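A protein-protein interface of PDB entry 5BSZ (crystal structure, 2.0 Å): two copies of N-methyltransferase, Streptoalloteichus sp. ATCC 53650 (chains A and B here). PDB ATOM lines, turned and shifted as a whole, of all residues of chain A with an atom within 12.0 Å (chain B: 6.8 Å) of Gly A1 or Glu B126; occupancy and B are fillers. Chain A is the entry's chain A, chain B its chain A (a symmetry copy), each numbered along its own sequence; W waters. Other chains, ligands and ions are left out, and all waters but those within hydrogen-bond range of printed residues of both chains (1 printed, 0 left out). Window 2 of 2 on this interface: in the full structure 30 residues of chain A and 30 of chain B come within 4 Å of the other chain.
The side-chain carboxylate (OE2) of Glu B126 is in hydrogen-bond range of the backbone NH (N) of Gly A1 (2.7 Å).
O of Tyr B120 lies within hydrogen-bond range of N of His A2 (2.8 Å).
The side-chain carboxylate (OD1) of Asp B98 lies close to the backbone NH (N) of Phe B100 (3.0 Å).
O of Phe B100 is in hydrogen-bond range of NH2 of Arg B129, 3.4 Å away.
The side-chain carboxylate of Glu B126 lies within hydrogen-bond range of the backbone NH of Ala B122 (2.7 Å).
The side-chain carboxylate (OD1) of Asp B123 lies within hydrogen-bond range of the backbone NH (N) of Glu B126, 2.8 Å away.
Gly A1 touches Phe B100.
Tyr B120 touches Gly A1.
His A2 touches Ala B121.
His A2 touches Ala B122 (NE2 to CA, 3.7 Å).
Of the printed residues of chain B, Gly A1 touches Phe B100, Tyr B120 and Glu B126.
Printed residues of chain B within 4 Å of His A2: Tyr B120 (2.8 Å), Ala B121 (3.96 Å) and Ala B122 (3.7 Å).
Val A5 touches none of the printed residues of chain B.
Printed residues of chain A within 4 Å of Tyr B120: Gly A1 (3.2 Å) and His A2 (2.8 Å).
Ala B121 touches just one residue of chain A: His A2.
No residue of chain A comes within 4 Å of Asp B123.
No residue of chain A comes within 4 Å of Thr B124.
Ala B125 touches none of the printed residues of chain A.
Glu B126 touches just one residue of chain A: Gly A1 (2.7 Å).
The nearest residue of chain B that does not touch Gly A1 is Ala B122 (4.3 Å).
The nearest residue of chain A that does not touch Glu B126 is His A2 (5.1 Å).
Printed residues of chain B that touch a printed residue of chain A: Phe B100, Tyr B120, Ala B121, Ala B122 and Glu B126.
Of the 5 printed residues of chain A, 2 touch a printed residue of chain B.
Printed residues of chain A that touch a printed residue of chain B: Gly A1 and His A2.
Hydrophobic or aromatic side chains of chain A within 4 Å of the printed part of chain B: His A2.
Among the printed residues, 6 pairs touch across the chains.
Among the printed residues, no Asp or Glu carboxylate lies within 4 Å of a Lys or Arg side-chain nitrogen of the other chain.
No position is printed for both chains.
Water W1 lies within hydrogen-bond range of the backbone carbonyl oxygen (O) of Ala B122 (2.6 Å) and a ring nitrogen (NE2) of His A2 (3.3 Å).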
ATOM      1  N   GLY A   1     -12.451  19.836  -7.585  1.00  0.00           N
ATOM      2  CA  GLY A   1     -13.312  21.034  -7.514  1.00  0.00           C
ATOM      3  C   GLY A   1     -13.636  21.604  -8.884  1.00  0.00           C
ATOM      4  O   GLY A   1     -13.191  21.101  -9.906  1.00  0.00           O
ATOM      5  N   HIS A   2     -14.414  22.673  -8.906  1.00  0.00           N
ATOM      6  CA  HIS A   2     -14.863  23.243 -10.195  1.00  0.00           C
ATOM      7  C   HIS A   2     -13.640  23.961 -10.819  1.00  0.00           C
ATOM      8  O   HIS A   2     -12.841  24.562 -10.102  1.00  0.00           O
ATOM      9  CB  HIS A   2     -15.929  24.275  -9.973  1.00  0.00           C
ATOM     10  CG  HIS A   2     -17.212  23.728  -9.477  1.00  0.00           C
ATOM     11  ND1 HIS A   2     -17.975  22.828 -10.184  1.00  0.00           N
ATOM     12  CD2 HIS A   2     -17.880  23.962  -8.322  1.00  0.00           C
ATOM     13  CE1 HIS A   2     -19.074  22.560  -9.508  1.00  0.00           C
ATOM     14  NE2 HIS A   2     -19.020  23.203  -8.359  1.00  0.00           N
ATOM     15  N   MET A   3     -13.470  23.844 -12.112  1.00  0.00           N
ATOM     16  CA  MET A   3     -12.355  24.454 -12.833  1.00  0.00           C
ATOM     17  C   MET A   3     -12.973  25.313 -13.963  1.00  0.00           C
ATOM     18  O   MET A   3     -13.719  24.803 -14.790  1.00  0.00           O
ATOM     19  CB  MET A   3     -11.448  23.400 -13.430  1.00  0.00           C
ATOM     20  CG  MET A   3     -10.452  23.950 -14.474  1.00  0.00           C
ATOM     21  SD  MET A   3      -9.169  24.955 -13.650  1.00  0.00           S
ATOM     22  CE  MET A   3      -8.121  23.638 -13.030  1.00  0.00           C
ATOM     23  N   ALA A   4     -12.715  26.611 -13.934  1.00  0.00           N
ATOM     24  CA  ALA A   4     -13.258  27.542 -14.932  1.00  0.00           C
ATOM     25  C   ALA A   4     -12.719  27.192 -16.325  1.00  0.00           C
ATOM     26  O   ALA A   4     -11.680  26.524 -16.477  1.00  0.00           O
ATOM     27  CB  ALA A   4     -12.865  28.967 -14.550  1.00  0.00           C
ATOM     28  N   VAL A   5     -13.442  27.638 -17.345  1.00  0.00           N
ATOM     29  CA  VAL A   5     -12.949  27.674 -18.706  1.00  0.00           C
ATOM     30  C   VAL A   5     -13.019  29.105 -19.236  1.00  0.00           C
ATOM     31  O   VAL A   5     -13.808  29.938 -18.762  1.00  0.00           O
ATOM     32  CB  VAL A   5     -13.760  26.810 -19.682  1.00  0.00           C
ATOM     33  CG1 VAL A   5     -13.570  25.324 -19.436  1.00  0.00           C
ATOM     34  CG2 VAL A   5     -15.240  27.149 -19.616  1.00  0.00           C
ATOM     35  N   ASP B  98      -3.107  22.958  -3.538  1.00  0.00           N
ATOM     36  CA  ASP B  98      -4.515  22.664  -3.692  1.00  0.00           C
ATOM     37  C   ASP B  98      -5.198  22.701  -2.325  1.00  0.00           C
ATOM     38  O   ASP B  98      -4.888  21.918  -1.405  1.00  0.00           O
ATOM     39  CB  ASP B  98      -4.671  21.301  -4.347  1.00  0.00           C
ATOM     40  CG  ASP B  98      -6.117  20.945  -4.626  1.00  0.00           C
ATOM     41  OD1 ASP B  98      -7.061  21.763  -4.381  1.00  0.00           O
ATOM     42  OD2 ASP B  98      -6.274  19.757  -4.964  1.00  0.00           O
ATOM     43  N   MET B  99      -6.151  23.614  -2.222  1.00  0.00           N
ATOM     44  CA  MET B  99      -6.894  23.836  -0.967  1.00  0.00           C
ATOM     45  C   MET B  99      -7.580  22.570  -0.516  1.00  0.00           C
ATOM     46  O   MET B  99      -7.902  22.430   0.663  1.00  0.00           O
ATOM     47  CB  MET B  99      -7.951  24.971  -1.124  1.00  0.00           C
ATOM     48  CG  MET B  99      -8.993  24.731  -2.198  1.00  0.00           C
ATOM     49  SD  MET B  99     -10.149  26.102  -2.657  1.00  0.00           S
ATOM     50  CE  MET B  99     -10.678  26.250  -1.003  1.00  0.00           C
ATOM     51  N   PHE B 100      -7.854  21.662  -1.446  1.00  0.00           N
ATOM     52  CA  PHE B 100      -8.570  20.439  -1.133  1.00  0.00           C
ATOM     53  C   PHE B 100      -7.737  19.391  -0.432  1.00  0.00           C
ATOM     54  O   PHE B 100      -8.300  18.500   0.200  1.00  0.00           O
ATOM     55  CB  PHE B 100      -9.241  19.840  -2.378  1.00  0.00           C
ATOM     56  CG  PHE B 100     -10.237  20.778  -2.940  1.00  0.00           C
ATOM     57  CD1 PHE B 100     -11.294  21.185  -2.150  1.00  0.00           C
ATOM     58  CD2 PHE B 100     -10.034  21.364  -4.163  1.00  0.00           C
ATOM     59  CE1 PHE B 100     -12.157  22.133  -2.614  1.00  0.00           C
ATOM     60  CE2 PHE B 100     -10.918  22.315  -4.632  1.00  0.00           C
ATOM     61  CZ  PHE B 100     -11.970  22.686  -3.857  1.00  0.00           C
ATOM     62  N   ILE B 118     -14.289  28.686  -0.934  1.00  0.00           N
ATOM     63  CA  ILE B 118     -14.442  27.307  -0.563  1.00  0.00           C
ATOM     64  C   ILE B 118     -15.437  26.556  -1.465  1.00  0.00           C
ATOM     65  O   ILE B 118     -15.359  25.348  -1.559  1.00  0.00           O
ATOM     66  CB  ILE B 118     -14.692  27.014   0.961  1.00  0.00           C
ATOM     67  CG1 ILE B 118     -14.113  25.599   1.300  1.00  0.00           C
ATOM     68  CG2 ILE B 118     -16.121  27.201   1.367  1.00  0.00           C
ATOM     69  CD1 ILE B 118     -13.907  25.332   2.764  1.00  0.00           C
ATOM     70  N   TYR B 120     -15.602  26.495  -4.628  1.00  0.00           N
ATOM     71  CA  TYR B 120     -15.030  25.628  -5.643  1.00  0.00           C
ATOM     72  C   TYR B 120     -15.203  24.131  -5.364  1.00  0.00           C
ATOM     73  O   TYR B 120     -15.159  23.336  -6.288  1.00  0.00           O
ATOM     74  CB  TYR B 120     -13.530  25.935  -5.837  1.00  0.00           C
ATOM     75  CG  TYR B 120     -13.183  27.208  -6.588  1.00  0.00           C
ATOM     76  CD1 TYR B 120     -12.675  27.163  -7.890  1.00  0.00           C
ATOM     77  CD2 TYR B 120     -13.381  28.433  -6.047  1.00  0.00           C
ATOM     78  CE1 TYR B 120     -12.325  28.315  -8.574  1.00  0.00           C
ATOM     79  CE2 TYR B 120     -13.068  29.594  -6.727  1.00  0.00           C
ATOM     80  CZ  TYR B 120     -12.559  29.535  -7.988  1.00  0.00           C
ATOM     81  OH  TYR B 120     -12.245  30.713  -8.598  1.00  0.00           O
ATOM     82  N   ALA B 121     -15.423  23.751  -4.104  1.00  0.00           N
ATOM     83  CA  ALA B 121     -15.747  22.375  -3.802  1.00  0.00           C
ATOM     84  C   ALA B 121     -16.986  21.999  -4.587  1.00  0.00           C
ATOM     85  O   ALA B 121     -17.962  22.735  -4.558  1.00  0.00           O
ATOM     86  CB  ALA B 121     -16.000  22.200  -2.310  1.00  0.00           C
ATOM     87  N   ALA B 122     -16.956  20.829  -5.200  1.00  0.00           N
ATOM     88  CA  ALA B 122     -18.054  20.421  -6.080  1.00  0.00           C
ATOM     89  C   ALA B 122     -19.200  19.712  -5.347  1.00  0.00           C
ATOM     90  O   ALA B 122     -20.312  19.694  -5.861  1.00  0.00           O
ATOM     91  CB  ALA B 122     -17.511  19.572  -7.207  1.00  0.00           C
ATOM     92  N   ASP B 123     -18.951  19.176  -4.150  1.00  0.00           N
ATOM     93  CA  ASP B 123     -19.969  18.415  -3.392  1.00  0.00           C
ATOM     94  C   ASP B 123     -19.562  18.410  -1.925  1.00  0.00           C
ATOM     95  O   ASP B 123     -18.482  18.911  -1.561  1.00  0.00           O
ATOM     96  CB  ASP B 123     -20.126  16.978  -3.917  1.00  0.00           C
ATOM     97  CG  ASP B 123     -18.791  16.221  -3.946  1.00  0.00           C
ATOM     98  OD1 ASP B 123     -18.000  16.277  -2.972  1.00  0.00           O
ATOM     99  OD2 ASP B 123     -18.482  15.595  -4.975  1.00  0.00           O
ATOM    100  N   THR B 124     -20.457  17.906  -1.088  1.00  0.00           N
ATOM    101  CA  THR B 124     -20.270  17.918   0.365  1.00  0.00           C
ATOM    102  C   THR B 124     -19.020  17.205   0.852  1.00  0.00           C
ATOM    103  O   THR B 124     -18.355  17.648   1.805  1.00  0.00           O
ATOM    104  CB  THR B 124     -21.526  17.306   1.028  1.00  0.00           C
ATOM    105  OG1 THR B 124     -22.653  18.086   0.619  1.00  0.00           O
ATOM    106  CG2 THR B 124     -21.427  17.407   2.514  1.00  0.00           C
ATOM    107  N   ALA B 125     -18.709  16.079   0.220  1.00  0.00           N
ATOM    108  CA  ALA B 125     -17.518  15.340   0.531  1.00  0.00           C
ATOM    109  C   ALA B 125     -16.271  16.190   0.278  1.00  0.00           C
ATOM    110  O   ALA B 125     -15.383  16.245   1.137  1.00  0.00           O
ATOM    111  CB  ALA B 125     -17.460  14.014  -0.235  1.00  0.00           C
ATOM    112  N   GLU B 126     -16.207  16.861  -0.872  1.00  0.00           N
ATOM    113  CA  GLU B 126     -15.084  17.738  -1.180  1.00  0.00           C
ATOM    114  C   GLU B 126     -14.995  18.972  -0.275  1.00  0.00           C
ATOM    115  O   GLU B 126     -13.895  19.386   0.165  1.00  0.00           O
ATOM    116  CB  GLU B 126     -15.133  18.176  -2.670  1.00  0.00           C
ATOM    117  CG  GLU B 126     -13.776  18.686  -3.129  1.00  0.00           C
ATOM    118  CD  GLU B 126     -13.695  18.865  -4.634  1.00  0.00           C
ATOM    119  OE1 GLU B 126     -14.745  19.202  -5.237  1.00  0.00           O
ATOM    120  OE2 GLU B 126     -12.574  18.717  -5.180  1.00  0.00           O
ATOM    121  N   LEU B 127     -16.144  19.524   0.092  1.00  0.00           N
ATOM    122  CA  LEU B 127     -16.192  20.577   1.076  1.00  0.00           C
ATOM    123  C   LEU B 127     -15.551  20.128   2.395  1.00  0.00           C
ATOM    124  O   LEU B 127     -14.674  20.826   2.966  1.00  0.00           O
ATOM    125  CB  LEU B 127     -17.645  21.033   1.290  1.00  0.00           C
ATOM    126  CG  LEU B 127     -17.960  22.078   2.332  1.00  0.00           C
ATOM    127  CD1 LEU B 127     -17.282  23.367   1.904  1.00  0.00           C
ATOM    128  CD2 LEU B 127     -19.454  22.241   2.579  1.00  0.00           C
ATOM    129  N   ALA B 128     -15.980  18.946   2.843  1.00  0.00           N
ATOM    130  CA  ALA B 128     -15.423  18.339   4.060  1.00  0.00           C
ATOM    131  C   ALA B 128     -13.930  18.134   3.936  1.00  0.00           C
ATOM    132  O   ALA B 128     -13.229  18.411   4.920  1.00  0.00           O
ATOM    133  CB  ALA B 128     -16.151  17.042   4.477  1.00  0.00           C
ATOM    134  N   ARG B 129     -13.417  17.736   2.774  1.00  0.00           N
ATOM    135  CA  ARG B 129     -11.974  17.564   2.615  1.00  0.00           C
ATOM    136  C   ARG B 129     -11.180  18.847   2.754  1.00  0.00           C
ATOM    137  O   ARG B 129     -10.136  18.867   3.439  1.00  0.00           O
ATOM    138  CB  ARG B 129     -11.592  16.905   1.286  1.00  0.00           C
ATOM    139  CG  ARG B 129     -11.024  15.513   1.476  1.00  0.00           C
ATOM    140  CD  ARG B 129     -11.013  14.716   0.184  1.00  0.00           C
ATOM    141  NE  ARG B 129     -10.351  15.477  -0.854  1.00  0.00           N
ATOM    142  CZ  ARG B 129      -9.085  15.319  -1.211  1.00  0.00           C
ATOM    143  NH1 ARG B 129      -8.311  14.425  -0.605  1.00  0.00           N
ATOM    144  NH2 ARG B 129      -8.613  16.080  -2.176  1.00  0.00           N
ATOM    145  N   ALA B 130     -11.653  19.910   2.085  1.00  0.00           N
ATOM    146  CA  ALA B 130     -11.061  21.254   2.259  1.00  0.00           C
ATOM    147  C   ALA B 130     -11.063  21.701   3.728  1.00  0.00           C
ATOM    148  O   ALA B 130     -10.123  22.282   4.211  1.00  0.00           O
ATOM    149  CB  ALA B 130     -11.785  22.317   1.433  1.00  0.00           C
ATOM    150  N   VAL B 131     -12.172  21.529   4.433  1.00  0.00           N
ATOM    151  CA  VAL B 131     -12.276  22.033   5.794  1.00  0.00           C
ATOM    152  C   VAL B 131     -11.372  21.212   6.713  1.00  0.00           C
ATOM    153  O   VAL B 131     -10.743  21.751   7.644  1.00  0.00           O
ATOM    154  CB  VAL B 131     -13.744  22.010   6.244  1.00  0.00           C
ATOM    155  CG1 VAL B 131     -13.862  22.352   7.715  1.00  0.00           C
ATOM    156  CG2 VAL B 131     -14.538  23.023   5.399  1.00  0.00           C
ATOM    157  N   ARG B 132     -11.288  19.919   6.436  1.00  0.00           N
ATOM    158  CA  ARG B 132     -10.331  19.092   7.163  1.00  0.00           C
ATOM    159  C   ARG B 132      -8.885  19.540   6.965  1.00  0.00           C
ATOM    160  O   ARG B 132      -8.071  19.589   7.920  1.00  0.00           O
ATOM    161  CB  ARG B 132     -10.520  17.631   6.781  1.00  0.00           C
ATOM    162  CG  ARG B 132     -10.142  16.641   7.872  1.00  0.00           C
ATOM    163  CD  ARG B 132     -11.173  15.492   7.992  1.00  0.00           C
ATOM    164  NE  ARG B 132     -11.701  15.104   6.676  1.00  0.00           N
ATOM    165  CZ  ARG B 132     -12.987  15.043   6.287  1.00  0.00           C
ATOM    166  NH1 ARG B 132     -14.023  15.296   7.126  1.00  0.00           N
ATOM    167  NH2 ARG B 132     -13.210  14.718   4.997  1.00  0.00           N
ATOM    168  N   PHE B 211     -24.082  25.540  -1.234  1.00  0.00           N
ATOM    169  CA  PHE B 211     -24.255  24.617  -0.102  1.00  0.00           C
ATOM    170  C   PHE B 211     -25.176  25.210   0.929  1.00  0.00           C
ATOM    171  O   PHE B 211     -25.058  26.395   1.270  1.00  0.00           O
ATOM    172  CB  PHE B 211     -22.939  24.300   0.612  1.00  0.00           C
ATOM    173  CG  PHE B 211     -21.926  23.592  -0.213  1.00  0.00           C
ATOM    174  CD1 PHE B 211     -20.825  24.256  -0.688  1.00  0.00           C
ATOM    175  CD2 PHE B 211     -22.023  22.227  -0.440  1.00  0.00           C
ATOM    176  CE1 PHE B 211     -19.874  23.582  -1.433  1.00  0.00           C
ATOM    177  CE2 PHE B 211     -21.075  21.549  -1.155  1.00  0.00           C
ATOM    178  CZ  PHE B 211     -19.963  22.218  -1.642  1.00  0.00           C
HETATM  179  O   HOH W   1     -21.438  21.075  -7.734  1.00  0.00           O
